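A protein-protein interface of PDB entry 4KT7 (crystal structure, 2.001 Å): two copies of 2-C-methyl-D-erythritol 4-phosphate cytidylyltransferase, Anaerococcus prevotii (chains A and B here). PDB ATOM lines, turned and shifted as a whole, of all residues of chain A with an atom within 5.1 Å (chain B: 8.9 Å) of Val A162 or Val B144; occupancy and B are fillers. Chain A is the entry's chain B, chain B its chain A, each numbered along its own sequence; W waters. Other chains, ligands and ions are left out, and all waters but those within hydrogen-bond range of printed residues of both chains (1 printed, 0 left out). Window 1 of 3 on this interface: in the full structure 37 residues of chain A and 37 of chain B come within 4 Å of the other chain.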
ATOM      1  N   THR A 138      -3.431 -11.297   5.160  1.00  0.00           N
ATOM      2  CA  THR A 138      -4.795 -11.656   4.809  1.00  0.00           C
ATOM      3  C   THR A 138      -5.034 -13.134   5.016  1.00  0.00           C
ATOM      4  O   THR A 138      -4.144 -13.961   4.766  1.00  0.00           O
ATOM      5  CB  THR A 138      -5.104 -11.342   3.348  1.00  0.00           C
ATOM      6  OG1 THR A 138      -4.133 -11.992   2.522  1.00  0.00           O
ATOM      7  CG2 THR A 138      -5.095  -9.848   3.106  1.00  0.00           C
ATOM      8  N   LYS A 139      -6.242 -13.475   5.449  1.00  0.00           N
ATOM      9  CA  LYS A 139      -6.570 -14.882   5.658  1.00  0.00           C
ATOM     10  C   LYS A 139      -6.388 -15.615   4.328  1.00  0.00           C
ATOM     11  O   LYS A 139      -6.852 -15.133   3.283  1.00  0.00           O
ATOM     12  CB  LYS A 139      -7.997 -15.031   6.159  1.00  0.00           C
ATOM     13  CG  LYS A 139      -8.406 -16.489   6.448  1.00  0.00           C
ATOM     14  CD  LYS A 139      -9.886 -16.570   6.806  1.00  0.00           C
ATOM     15  CE  LYS A 139     -10.185 -15.699   8.009  1.00  0.00           C
ATOM     16  NZ  LYS A 139     -11.574 -15.904   8.519  1.00  0.00           N
ATOM     17  N   SER A 140      -5.680 -16.743   4.354  1.00  0.00           N
ATOM     18  CA  SER A 140      -5.379 -17.466   3.122  1.00  0.00           C
ATOM     19  C   SER A 140      -6.661 -18.002   2.524  1.00  0.00           C
ATOM     20  O   SER A 140      -7.460 -18.650   3.217  1.00  0.00           O
ATOM     21  CB  SER A 140      -4.410 -18.641   3.372  1.00  0.00           C
ATOM     22  OG  SER A 140      -4.319 -19.464   2.205  1.00  0.00           O
ATOM     23  N   VAL A 144      -4.243 -24.402   3.581  1.00  0.00           N
ATOM     24  CA  VAL A 144      -2.867 -24.764   3.921  1.00  0.00           C
ATOM     25  C   VAL A 144      -2.846 -26.081   4.687  1.00  0.00           C
ATOM     26  O   VAL A 144      -3.772 -26.371   5.469  1.00  0.00           O
ATOM     27  CB  VAL A 144      -2.176 -23.650   4.750  1.00  0.00           C
ATOM     28  CG1 VAL A 144      -0.896 -24.166   5.463  1.00  0.00           C
ATOM     29  CG2 VAL A 144      -1.852 -22.458   3.852  1.00  0.00           C
ATOM     30  N   PRO A 157      -3.990 -26.873   9.688  1.00  0.00           N
ATOM     31  CA  PRO A 157      -4.288 -25.886  10.737  1.00  0.00           C
ATOM     32  C   PRO A 157      -5.697 -25.351  10.566  1.00  0.00           C
ATOM     33  O   PRO A 157      -6.226 -25.408   9.447  1.00  0.00           O
ATOM     34  CB  PRO A 157      -3.306 -24.735  10.443  1.00  0.00           C
ATOM     35  CG  PRO A 157      -2.323 -25.268   9.481  1.00  0.00           C
ATOM     36  CD  PRO A 157      -3.003 -26.398   8.723  1.00  0.00           C
ATOM     37  N   ASN A 158      -6.284 -24.818  11.632  1.00  0.00           N
ATOM     38  CA  ASN A 158      -7.561 -24.125  11.531  1.00  0.00           C
ATOM     39  C   ASN A 158      -7.450 -22.972  10.525  1.00  0.00           C
ATOM     40  O   ASN A 158      -6.658 -22.034  10.711  1.00  0.00           O
ATOM     41  CB  ASN A 158      -7.964 -23.602  12.910  1.00  0.00           C
ATOM     42  CG  ASN A 158      -9.367 -23.028  12.936  1.00  0.00           C
ATOM     43  OD1 ASN A 158      -9.835 -22.445  11.952  1.00  0.00           O
ATOM     44  ND2 ASN A 158     -10.049 -23.183  14.070  1.00  0.00           N
ATOM     45  N   ARG A 159      -8.255 -23.019   9.466  1.00  0.00           N
ATOM     46  CA  ARG A 159      -8.099 -22.054   8.372  1.00  0.00           C
ATOM     47  C   ARG A 159      -8.422 -20.606   8.771  1.00  0.00           C
ATOM     48  O   ARG A 159      -7.993 -19.671   8.116  1.00  0.00           O
ATOM     49  CB  ARG A 159      -8.938 -22.477   7.151  1.00  0.00           C
ATOM     50  CG  ARG A 159     -10.422 -22.551   7.437  1.00  0.00           C
ATOM     51  CD  ARG A 159     -11.240 -22.678   6.148  1.00  0.00           C
ATOM     52  NE  ARG A 159     -11.270 -21.424   5.399  1.00  0.00           N
ATOM     53  CZ  ARG A 159     -12.093 -20.410   5.663  1.00  0.00           C
ATOM     54  NH1 ARG A 159     -12.041 -19.307   4.929  1.00  0.00           N
ATOM     55  NH2 ARG A 159     -12.968 -20.495   6.661  1.00  0.00           N
ATOM     56  N   ASP A 160      -9.168 -20.415   9.849  1.00  0.00           N
ATOM     57  CA  ASP A 160      -9.496 -19.054  10.275  1.00  0.00           C
ATOM     58  C   ASP A 160      -8.285 -18.342  10.876  1.00  0.00           C
ATOM     59  O   ASP A 160      -8.320 -17.137  11.123  1.00  0.00           O
ATOM     60  CB  ASP A 160     -10.651 -19.074  11.267  1.00  0.00           C
ATOM     61  CG  ASP A 160     -11.973 -19.456  10.608  1.00  0.00           C
ATOM     62  OD1 ASP A 160     -12.181 -19.048   9.441  1.00  0.00           O
ATOM     63  OD2 ASP A 160     -12.788 -20.160  11.248  1.00  0.00           O
ATOM     64  N   TYR A 161      -7.204 -19.082  11.095  1.00  0.00           N
ATOM     65  CA  TYR A 161      -6.048 -18.493  11.747  1.00  0.00           C
ATOM     66  C   TYR A 161      -4.811 -18.531  10.884  1.00  0.00           C
ATOM     67  O   TYR A 161      -3.727 -18.180  11.347  1.00  0.00           O
ATOM     68  CB  TYR A 161      -5.810 -19.152  13.113  1.00  0.00           C
ATOM     69  CG  TYR A 161      -6.973 -18.946  14.051  1.00  0.00           C
ATOM     70  CD1 TYR A 161      -7.260 -17.693  14.574  1.00  0.00           C
ATOM     71  CD2 TYR A 161      -7.800 -19.999  14.396  1.00  0.00           C
ATOM     72  CE1 TYR A 161      -8.337 -17.502  15.433  1.00  0.00           C
ATOM     73  CE2 TYR A 161      -8.876 -19.816  15.246  1.00  0.00           C
ATOM     74  CZ  TYR A 161      -9.140 -18.570  15.760  1.00  0.00           C
ATOM     75  OH  TYR A 161     -10.212 -18.393  16.606  1.00  0.00           O
ATOM     76  N   VAL A 162      -4.978 -18.964   9.632  1.00  0.00           N
ATOM     77  CA  VAL A 162      -3.875 -19.022   8.674  1.00  0.00           C
ATOM     78  C   VAL A 162      -3.854 -17.770   7.807  1.00  0.00           C
ATOM     79  O   VAL A 162      -4.769 -17.540   7.025  1.00  0.00           O
ATOM     80  CB  VAL A 162      -3.988 -20.249   7.748  1.00  0.00           C
ATOM     81  CG1 VAL A 162      -2.865 -20.245   6.713  1.00  0.00           C
ATOM     82  CG2 VAL A 162      -3.941 -21.542   8.582  1.00  0.00           C
ATOM     83  N   TYR A 163      -2.794 -16.973   7.941  1.00  0.00           N
ATOM     84  CA  TYR A 163      -2.710 -15.704   7.218  1.00  0.00           C
ATOM     85  C   TYR A 163      -1.459 -15.595   6.356  1.00  0.00           C
ATOM     86  O   TYR A 163      -0.379 -16.051   6.744  1.00  0.00           O
ATOM     87  CB  TYR A 163      -2.768 -14.544   8.217  1.00  0.00           C
ATOM     88  CG  TYR A 163      -4.175 -14.161   8.660  1.00  0.00           C
ATOM     89  CD1 TYR A 163      -4.951 -15.029   9.402  1.00  0.00           C
ATOM     90  CD2 TYR A 163      -4.712 -12.919   8.339  1.00  0.00           C
ATOM     91  CE1 TYR A 163      -6.231 -14.684   9.807  1.00  0.00           C
ATOM     92  CE2 TYR A 163      -5.983 -12.554   8.748  1.00  0.00           C
ATOM     93  CZ  TYR A 163      -6.735 -13.436   9.481  1.00  0.00           C
ATOM     94  OH  TYR A 163      -7.996 -13.073   9.876  1.00  0.00           O
ATOM     95  N   ASN A 164      -1.608 -14.989   5.178  1.00  0.00           N
ATOM     96  CA  ASN A 164      -0.469 -14.693   4.299  1.00  0.00           C
ATOM     97  C   ASN A 164      -0.019 -13.241   4.495  1.00  0.00           C
ATOM     98  O   ASN A 164      -0.834 -12.333   4.361  1.00  0.00           O
ATOM     99  CB  ASN A 164      -0.894 -14.866   2.844  1.00  0.00           C
ATOM    100  CG  ASN A 164      -1.224 -16.317   2.502  1.00  0.00           C
ATOM    101  OD1 ASN A 164      -0.436 -17.221   2.783  1.00  0.00           O
ATOM    102  ND2 ASN A 164      -2.377 -16.540   1.888  1.00  0.00           N
ATOM    103  N   THR B 138       1.340 -27.457  -3.204  1.00  0.00           N
ATOM    104  CA  THR B 138       2.541 -26.712  -3.603  1.00  0.00           C
ATOM    105  C   THR B 138       3.068 -25.903  -2.431  1.00  0.00           C
ATOM    106  O   THR B 138       2.278 -25.344  -1.654  1.00  0.00           O
ATOM    107  CB  THR B 138       2.290 -25.736  -4.764  1.00  0.00           C
ATOM    108  OG1 THR B 138       1.179 -24.878  -4.448  1.00  0.00           O
ATOM    109  CG2 THR B 138       2.051 -26.490  -6.093  1.00  0.00           C
ATOM    110  N   LYS B 139       4.394 -25.841  -2.303  1.00  0.00           N
ATOM    111  CA  LYS B 139       4.985 -25.087  -1.214  1.00  0.00           C
ATOM    112  C   LYS B 139       4.513 -23.648  -1.332  1.00  0.00           C
ATOM    113  O   LYS B 139       4.501 -23.078  -2.430  1.00  0.00           O
ATOM    114  CB  LYS B 139       6.507 -25.134  -1.244  1.00  0.00           C
ATOM    115  CG  LYS B 139       7.127 -24.429  -0.038  1.00  0.00           C
ATOM    116  CD  LYS B 139       8.653 -24.487  -0.089  1.00  0.00           C
ATOM    117  CE  LYS B 139       9.154 -25.849   0.378  1.00  0.00           C
ATOM    118  NZ  LYS B 139      10.568 -26.055  -0.045  1.00  0.00           N
ATOM    119  N   SER B 140       4.081 -23.068  -0.219  1.00  0.00           N
ATOM    120  CA  SER B 140       3.533 -21.722  -0.285  1.00  0.00           C
ATOM    121  C   SER B 140       4.647 -20.749  -0.593  1.00  0.00           C
ATOM    122  O   SER B 140       5.688 -20.727   0.090  1.00  0.00           O
ATOM    123  CB  SER B 140       2.842 -21.334   1.028  1.00  0.00           C
ATOM    124  OG  SER B 140       2.460 -19.968   0.978  1.00  0.00           O
ATOM    125  N   LYS B 141       4.438 -19.973  -1.647  1.00  0.00           N
ATOM    126  CA  LYS B 141       5.338 -18.892  -1.988  1.00  0.00           C
ATOM    127  C   LYS B 141       5.114 -17.662  -1.114  1.00  0.00           C
ATOM    128  O   LYS B 141       6.031 -16.886  -0.916  1.00  0.00           O
ATOM    129  CB  LYS B 141       5.184 -18.520  -3.464  1.00  0.00           C
ATOM    130  CG  LYS B 141       5.912 -19.446  -4.411  1.00  0.00           C
ATOM    131  CD  LYS B 141       5.824 -18.914  -5.859  1.00  0.00           C
ATOM    132  CE  LYS B 141       6.533 -19.849  -6.836  1.00  0.00           C
ATOM    133  NZ  LYS B 141       6.414 -19.435  -8.270  1.00  0.00           N
ATOM    134  N   ASP B 142       3.899 -17.470  -0.609  1.00  0.00           N
ATOM    135  CA  ASP B 142       3.639 -16.380   0.337  1.00  0.00           C
ATOM    136  C   ASP B 142       3.920 -16.861   1.755  1.00  0.00           C
ATOM    137  O   ASP B 142       3.611 -17.994   2.095  1.00  0.00           O
ATOM    138  CB  ASP B 142       2.183 -15.927   0.256  1.00  0.00           C
ATOM    139  CG  ASP B 142       1.880 -15.169  -1.010  1.00  0.00           C
ATOM    140  OD1 ASP B 142       2.412 -14.049  -1.167  1.00  0.00           O
ATOM    141  OD2 ASP B 142       1.104 -15.691  -1.842  1.00  0.00           O
ATOM    142  N   THR B 143       4.492 -16.006   2.593  1.00  0.00           N
ATOM    143  CA  THR B 143       4.823 -16.445   3.948  1.00  0.00           C
ATOM    144  C   THR B 143       3.595 -16.495   4.838  1.00  0.00           C
ATOM    145  O   THR B 143       2.890 -15.494   4.998  1.00  0.00           O
ATOM    146  CB  THR B 143       5.860 -15.526   4.603  1.00  0.00           C
ATOM    147  OG1 THR B 143       7.083 -15.599   3.868  1.00  0.00           O
ATOM    148  CG2 THR B 143       6.109 -15.936   6.059  1.00  0.00           C
ATOM    149  N   VAL B 144       3.363 -17.662   5.438  1.00  0.00           N
ATOM    150  CA  VAL B 144       2.220 -17.897   6.312  1.00  0.00           C
ATOM    151  C   VAL B 144       2.520 -17.616   7.791  1.00  0.00           C
ATOM    152  O   VAL B 144       3.612 -17.925   8.274  1.00  0.00           O
ATOM    153  CB  VAL B 144       1.755 -19.361   6.187  1.00  0.00           C
ATOM    154  CG1 VAL B 144       0.766 -19.711   7.287  1.00  0.00           C
ATOM    155  CG2 VAL B 144       1.129 -19.578   4.819  1.00  0.00           C
ATOM    156  N   LYS B 145       1.556 -17.014   8.499  1.00  0.00           N
ATOM    157  CA  LYS B 145       1.632 -16.901   9.958  1.00  0.00           C
ATOM    158  C   LYS B 145       0.393 -17.543  10.536  1.00  0.00           C
ATOM    159  O   LYS B 145      -0.682 -17.451   9.942  1.00  0.00           O
ATOM    160  CB  LYS B 145       1.654 -15.436  10.418  1.00  0.00           C
ATOM    161  CG  LYS B 145       2.750 -14.577   9.800  1.00  0.00           C
ATOM    162  CD  LYS B 145       3.992 -14.469  10.660  1.00  0.00           C
ATOM    163  CE  LYS B 145       4.966 -13.466  10.035  1.00  0.00           C
ATOM    164  NZ  LYS B 145       6.245 -13.396  10.815  1.00  0.00           N
ATOM    165  N   ILE B 146       0.536 -18.169  11.699  1.00  0.00           N
ATOM    166  CA  ILE B 146      -0.617 -18.548  12.501  1.00  0.00           C
ATOM    167  C   ILE B 146      -0.888 -17.423  13.492  1.00  0.00           C
ATOM    168  O   ILE B 146       0.014 -17.004  14.221  1.00  0.00           O
ATOM    169  CB  ILE B 146      -0.340 -19.836  13.296  1.00  0.00           C
ATOM    170  CG1 ILE B 146       0.014 -20.975  12.340  1.00  0.00           C
ATOM    171  CG2 ILE B 146      -1.559 -20.210  14.140  1.00  0.00           C
ATOM    172  CD1 ILE B 146      -1.023 -21.173  11.269  1.00  0.00           C
ATOM    173  N   ILE B 147      -2.120 -16.914  13.523  1.00  0.00           N
ATOM    174  CA  ILE B 147      -2.430 -15.775  14.383  1.00  0.00           C
ATOM    175  C   ILE B 147      -3.504 -16.178  15.404  1.00  0.00           C
ATOM    176  O   ILE B 147      -4.120 -17.230  15.257  1.00  0.00           O
ATOM    177  CB  ILE B 147      -2.919 -14.589  13.551  1.00  0.00           C
ATOM    178  CG1 ILE B 147      -4.342 -14.856  13.085  1.00  0.00           C
ATOM    179  CG2 ILE B 147      -2.005 -14.369  12.319  1.00  0.00           C
ATOM    180  CD1 ILE B 147      -5.133 -13.614  12.850  1.00  0.00           C
ATOM    181  N   ASP B 148      -3.740 -15.355  16.427  1.00  0.00           N
ATOM    182  CA  ASP B 148      -4.758 -15.693  17.441  1.00  0.00           C
ATOM    183  C   ASP B 148      -6.027 -14.862  17.306  1.00  0.00           C
ATOM    184  O   ASP B 148      -6.156 -14.073  16.365  1.00  0.00           O
ATOM    185  CB  ASP B 148      -4.193 -15.604  18.869  1.00  0.00           C
ATOM    186  CG  ASP B 148      -3.758 -14.199  19.256  1.00  0.00           C
ATOM    187  OD1 ASP B 148      -4.281 -13.205  18.702  1.00  0.00           O
ATOM    188  OD2 ASP B 148      -2.888 -14.079  20.151  1.00  0.00           O
ATOM    189  N   VAL B 153       0.278 -12.274  16.142  1.00  0.00           N
ATOM    190  CA  VAL B 153       0.969 -13.447  15.636  1.00  0.00           C
ATOM    191  C   VAL B 153       1.204 -14.469  16.757  1.00  0.00           C
ATOM    192  O   VAL B 153       1.797 -14.146  17.801  1.00  0.00           O
ATOM    193  CB  VAL B 153       2.322 -13.052  14.987  1.00  0.00           C
ATOM    194  CG1 VAL B 153       3.150 -14.300  14.623  1.00  0.00           C
ATOM    195  CG2 VAL B 153       2.071 -12.202  13.753  1.00  0.00           C
ATOM    196  N   PHE B 155       2.743 -17.728  15.899  1.00  0.00           N
ATOM    197  CA  PHE B 155       4.089 -18.105  15.469  1.00  0.00           C
ATOM    198  C   PHE B 155       4.157 -18.201  13.946  1.00  0.00           C
ATOM    199  O   PHE B 155       3.125 -18.197  13.258  1.00  0.00           O
ATOM    200  CB  PHE B 155       4.503 -19.446  16.106  1.00  0.00           C
ATOM    201  CG  PHE B 155       3.741 -20.630  15.565  1.00  0.00           C
ATOM    202  CD1 PHE B 155       2.442 -20.862  15.954  1.00  0.00           C
ATOM    203  CD2 PHE B 155       4.319 -21.488  14.647  1.00  0.00           C
ATOM    204  CE1 PHE B 155       1.735 -21.941  15.455  1.00  0.00           C
ATOM    205  CE2 PHE B 155       3.619 -22.578  14.146  1.00  0.00           C
ATOM    206  CZ  PHE B 155       2.324 -22.795  14.542  1.00  0.00           C
ATOM    207  N   THR B 156       5.377 -18.261  13.423  1.00  0.00           N
ATOM    208  CA  THR B 156       5.595 -18.427  12.001  1.00  0.00           C
ATOM    209  C   THR B 156       5.992 -19.868  11.768  1.00  0.00           C
ATOM    210  O   THR B 156       7.036 -20.305  12.255  1.00  0.00           O
ATOM    211  CB  THR B 156       6.743 -17.540  11.497  1.00  0.00           C
ATOM    212  OG1 THR B 156       6.544 -16.192  11.942  1.00  0.00           O
ATOM    213  CG2 THR B 156       6.812 -17.564   9.973  1.00  0.00           C
ATOM    214  N   PRO B 157       5.161 -20.621  11.031  1.00  0.00           N
ATOM    215  CA  PRO B 157       5.507 -22.025  10.806  1.00  0.00           C
ATOM    216  C   PRO B 157       6.755 -22.103   9.966  1.00  0.00           C
ATOM    217  O   PRO B 157       7.048 -21.167   9.212  1.00  0.00           O
ATOM    218  CB  PRO B 157       4.321 -22.564   9.994  1.00  0.00           C
ATOM    219  CG  PRO B 157       3.193 -21.624  10.287  1.00  0.00           C
ATOM    220  CD  PRO B 157       3.834 -20.279  10.494  1.00  0.00           C
ATOM    221  N   ASN B 158       7.494 -23.195  10.119  1.00  0.00           N
ATOM    222  CA  ASN B 158       8.653 -23.461   9.288  1.00  0.00           C
ATOM    223  C   ASN B 158       8.193 -23.448   7.836  1.00  0.00           C
ATOM    224  O   ASN B 158       7.366 -24.263   7.448  1.00  0.00           O
ATOM    225  CB  ASN B 158       9.218 -24.841   9.644  1.00  0.00           C
ATOM    226  CG  ASN B 158      10.506 -25.141   8.926  1.00  0.00           C
ATOM    227  OD1 ASN B 158      10.803 -24.543   7.880  1.00  0.00           O
ATOM    228  ND2 ASN B 158      11.296 -26.063   9.484  1.00  0.00           N
ATOM    229  N   ARG B 159       8.727 -22.522   7.048  1.00  0.00           N
ATOM    230  CA  ARG B 159       8.285 -22.282   5.663  1.00  0.00           C
ATOM    231  C   ARG B 159       8.436 -23.436   4.697  1.00  0.00           C
ATOM    232  O   ARG B 159       7.688 -23.522   3.713  1.00  0.00           O
ATOM    233  CB  ARG B 159       9.044 -21.102   5.073  1.00  0.00           C
ATOM    234  CG  ARG B 159       8.204 -19.869   4.901  1.00  0.00           C
ATOM    235  CD  ARG B 159       8.957 -18.826   4.110  1.00  0.00           C
ATOM    236  NE  ARG B 159       8.096 -18.118   3.165  1.00  0.00           N
ATOM    237  CZ  ARG B 159       8.221 -18.198   1.843  1.00  0.00           C
ATOM    238  NH1 ARG B 159       9.172 -18.954   1.305  1.00  0.00           N
ATOM    239  NH2 ARG B 159       7.398 -17.516   1.059  1.00  0.00           N
ATOM    240  N   TYR B 161       7.692 -26.379   5.130  1.00  0.00           N
ATOM    241  CA  TYR B 161       6.671 -27.401   5.338  1.00  0.00           C
ATOM    242  C   TYR B 161       5.247 -26.860   5.200  1.00  0.00           C
ATOM    243  O   TYR B 161       4.280 -27.544   5.543  1.00  0.00           O
ATOM    244  CB  TYR B 161       6.894 -28.089   6.693  1.00  0.00           C
ATOM    245  CG  TYR B 161       8.247 -28.755   6.779  1.00  0.00           C
ATOM    246  CD1 TYR B 161       8.545 -29.855   5.996  1.00  0.00           C
ATOM    247  CD2 TYR B 161       9.239 -28.266   7.621  1.00  0.00           C
ATOM    248  CE1 TYR B 161       9.801 -30.468   6.059  1.00  0.00           C
ATOM    249  CE2 TYR B 161      10.506 -28.874   7.690  1.00  0.00           C
ATOM    250  CZ  TYR B 161      10.770 -29.975   6.899  1.00  0.00           C
ATOM    251  OH  TYR B 161      11.996 -30.605   6.938  1.00  0.00           O
ATOM    252  N   VAL B 162       5.129 -25.632   4.690  1.00  0.00           N
ATOM    253  CA  VAL B 162       3.832 -24.987   4.479  1.00  0.00           C
ATOM    254  C   VAL B 162       3.377 -25.116   3.010  1.00  0.00           C
ATOM    255  O   VAL B 162       4.000 -24.553   2.119  1.00  0.00           O
ATOM    256  CB  VAL B 162       3.883 -23.476   4.853  1.00  0.00           C
ATOM    257  CG1 VAL B 162       2.519 -22.848   4.651  1.00  0.00           C
ATOM    258  CG2 VAL B 162       4.375 -23.276   6.317  1.00  0.00           C
ATOM    259  N   TYR B 163       2.305 -25.866   2.770  1.00  0.00           N
ATOM    260  CA  TYR B 163       1.811 -26.120   1.413  1.00  0.00           C
ATOM    261  C   TYR B 163       0.354 -25.740   1.206  1.00  0.00           C
ATOM    262  O   TYR B 163      -0.480 -25.920   2.088  1.00  0.00           O
ATOM    263  CB  TYR B 163       1.963 -27.600   1.046  1.00  0.00           C
ATOM    264  CG  TYR B 163       3.369 -28.029   0.719  1.00  0.00           C
ATOM    265  CD1 TYR B 163       4.405 -27.870   1.639  1.00  0.00           C
ATOM    266  CD2 TYR B 163       3.668 -28.607  -0.502  1.00  0.00           C
ATOM    267  CE1 TYR B 163       5.705 -28.266   1.336  1.00  0.00           C
ATOM    268  CE2 TYR B 163       4.962 -29.016  -0.811  1.00  0.00           C
ATOM    269  CZ  TYR B 163       5.969 -28.850   0.111  1.00  0.00           C
ATOM    270  OH  TYR B 163       7.238 -29.272  -0.202  1.00  0.00           O
ATOM    271  N   ASN B 164       0.053 -25.224   0.018  1.00  0.00           N
ATOM    272  CA  ASN B 164      -1.314 -24.920  -0.368  1.00  0.00           C
ATOM    273  C   ASN B 164      -1.833 -26.085  -1.182  1.00  0.00           C
ATOM    274  O   ASN B 164      -1.195 -26.463  -2.159  1.00  0.00           O
ATOM    275  CB  ASN B 164      -1.338 -23.669  -1.252  1.00  0.00           C
ATOM    276  CG  ASN B 164      -0.784 -22.443  -0.545  1.00  0.00           C
ATOM    277  OD1 ASN B 164       0.191 -21.826  -0.994  1.00  0.00           O
ATOM    278  ND2 ASN B 164      -1.413 -22.075   0.553  1.00  0.00           N
ATOM    279  N   THR B 191     -12.177 -28.915   5.409  1.00  0.00           N
ATOM    280  CA  THR B 191     -11.606 -28.029   4.398  1.00  0.00           C
ATOM    281  C   THR B 191     -11.498 -28.765   3.062  1.00  0.00           C
ATOM    282  O   THR B 191     -11.629 -28.151   2.009  1.00  0.00           O
ATOM    283  CB  THR B 191     -10.220 -27.497   4.808  1.00  0.00           C
ATOM    284  OG1 THR B 191      -9.333 -28.598   5.082  1.00  0.00           O
ATOM    285  CG2 THR B 191     -10.341 -26.617   6.034  1.00  0.00           C
HETATM  286  O   HOH W   1      -0.906 -19.442   1.770  1.00  0.00           O
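The backbone NH (N) of Lys B145 is in hydrogen-bond range of the backbone carbonyl oxygen (O) of Tyr A163 (2.8 Å).
The backbone NH of Ile B147 sits at hydrogen-bond distance from the backbone carbonyl oxygen of Tyr A161 (3.0 Å).
The backbone carbonyl oxygen (O) of Tyr A161 sits close to the backbone carbonyl oxygen (O) of Lys B145 (3.4 Å).
The backbone NH (N) of Asn B164 sits at hydrogen-bond distance from the backbone carbonyl oxygen (O) of Thr B138 (2.8 Å).
The backbone carbonyl oxygen (O) of Asp B142 sits at hydrogen-bond distance from the side-chain hydroxyl (OG) of Ser B140, at 2.5 Å.
OG1 of Thr B143 lies within hydrogen-bond range of NE of Arg B159, 2.8 Å away.
The backbone carbonyl oxygen (O) of Phe B155 sits at hydrogen-bond distance from the backbone NH (N) of Ile B146 (3.0 Å).
O of Thr A138 sits at hydrogen-bond distance from N of Asn A164 (2.8 Å).
O of Val A162 sits at hydrogen-bond distance from N of Ser A140 (2.9 Å).
Among the printed residues, merely in contact across the chains: Tyr A163 with Val B144 (3.2 Å), Val A144 with Tyr B163 (3.2 Å), Tyr A161 with Ile B146 (3.3 Å), Val A144 with Asn B164 (3.4 Å), Tyr A163 with Ile B147 (3.4 Å), Asn A164 with Val B144 (3.5 Å), Asn A164 with Thr B143 (3.5 Å), Val A162 with Val B144 (3.7 Å), Tyr A163 with Thr B143 (3.7 Å), Val A144 with Val B162 (3.7 Å), Val A162 with Lys B145 (3.8 Å), Asn A164 with Asp B142 (3.9 Å), Tyr A161 with Asp B148 (3.98 Å) and Val A162 with Ile B146 (3.98 Å).
Printed residues of chain B within 4 Å of Val A144: Val B162 (3.7 Å), Tyr B163 (3.2 Å) and Asn B164 (3.4 Å).
Ser B140 touches none of the printed residues of chain A.
Val B144 touches just these residues of chain A: Val A162, Tyr A163 and Asn A164.
Of the printed residues of chain A, Asp B148 touches Tyr A161 (3.98 Å).
Of the printed residues of chain A, Val B162 touches Val A144.
Printed residues of chain A within 4 Å of Tyr B163: Val A144.
Printed residues of chain A within 4 Å of Asn B164: Val A144.
The nearest printed residue of chain B that does not touch Val A162 is Ile B147 (5.2 Å).
The nearest printed residue of chain B that does not touch Tyr A163 is Ile B146 (5.2 Å).
Hydrophobic or aromatic side chains of chain B within 4 Å of the printed part of chain A: Val B144, Ile B146, Ile B147 and Val B162.
Of the 12 printed residues of chain A, 5 touch a printed residue of chain B.
Printed residues of chain A that touch a printed residue of chain B: Val A144, Tyr A161, Val A162, Tyr A163 and Asn A164.
Hydrophobic or aromatic side chains of chain A within 4 Å of the printed part of chain B: Val A144, Tyr A161, Val A162 and Tyr A163.
Along chain A the printed residues that touch a printed residue of chain B span positions 144 to 164.
Among the printed residues, 17 pairs touch across the chains.
Among the printed residues, no Asp or Glu carboxylate lies within 4 Å of a Lys or Arg side-chain nitrogen of the other chain.
Val A144 touches Val B162, and with the chains exchanged Val A162 touches Val B144.
Val A144 touches Tyr B163, and with the chains exchanged Tyr A163 touches Val B144.
Val A144 touches Asn B164, and with the chains exchanged Asn A164 touches Val B144.
11 positions are printed for both chains.
Water W1 lies within hydrogen-bond range of the side-chain amide oxygen (OD1) of Asn A164 (2.5 Å), the side-chain amide nitrogen (ND2) of Asn B164 (2.9 Å), the side-chain hydroxyl (OG) of Ser A140 (3.4 Å) and the side-chain hydroxyl (OG) of Ser B140 (3.5 Å).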
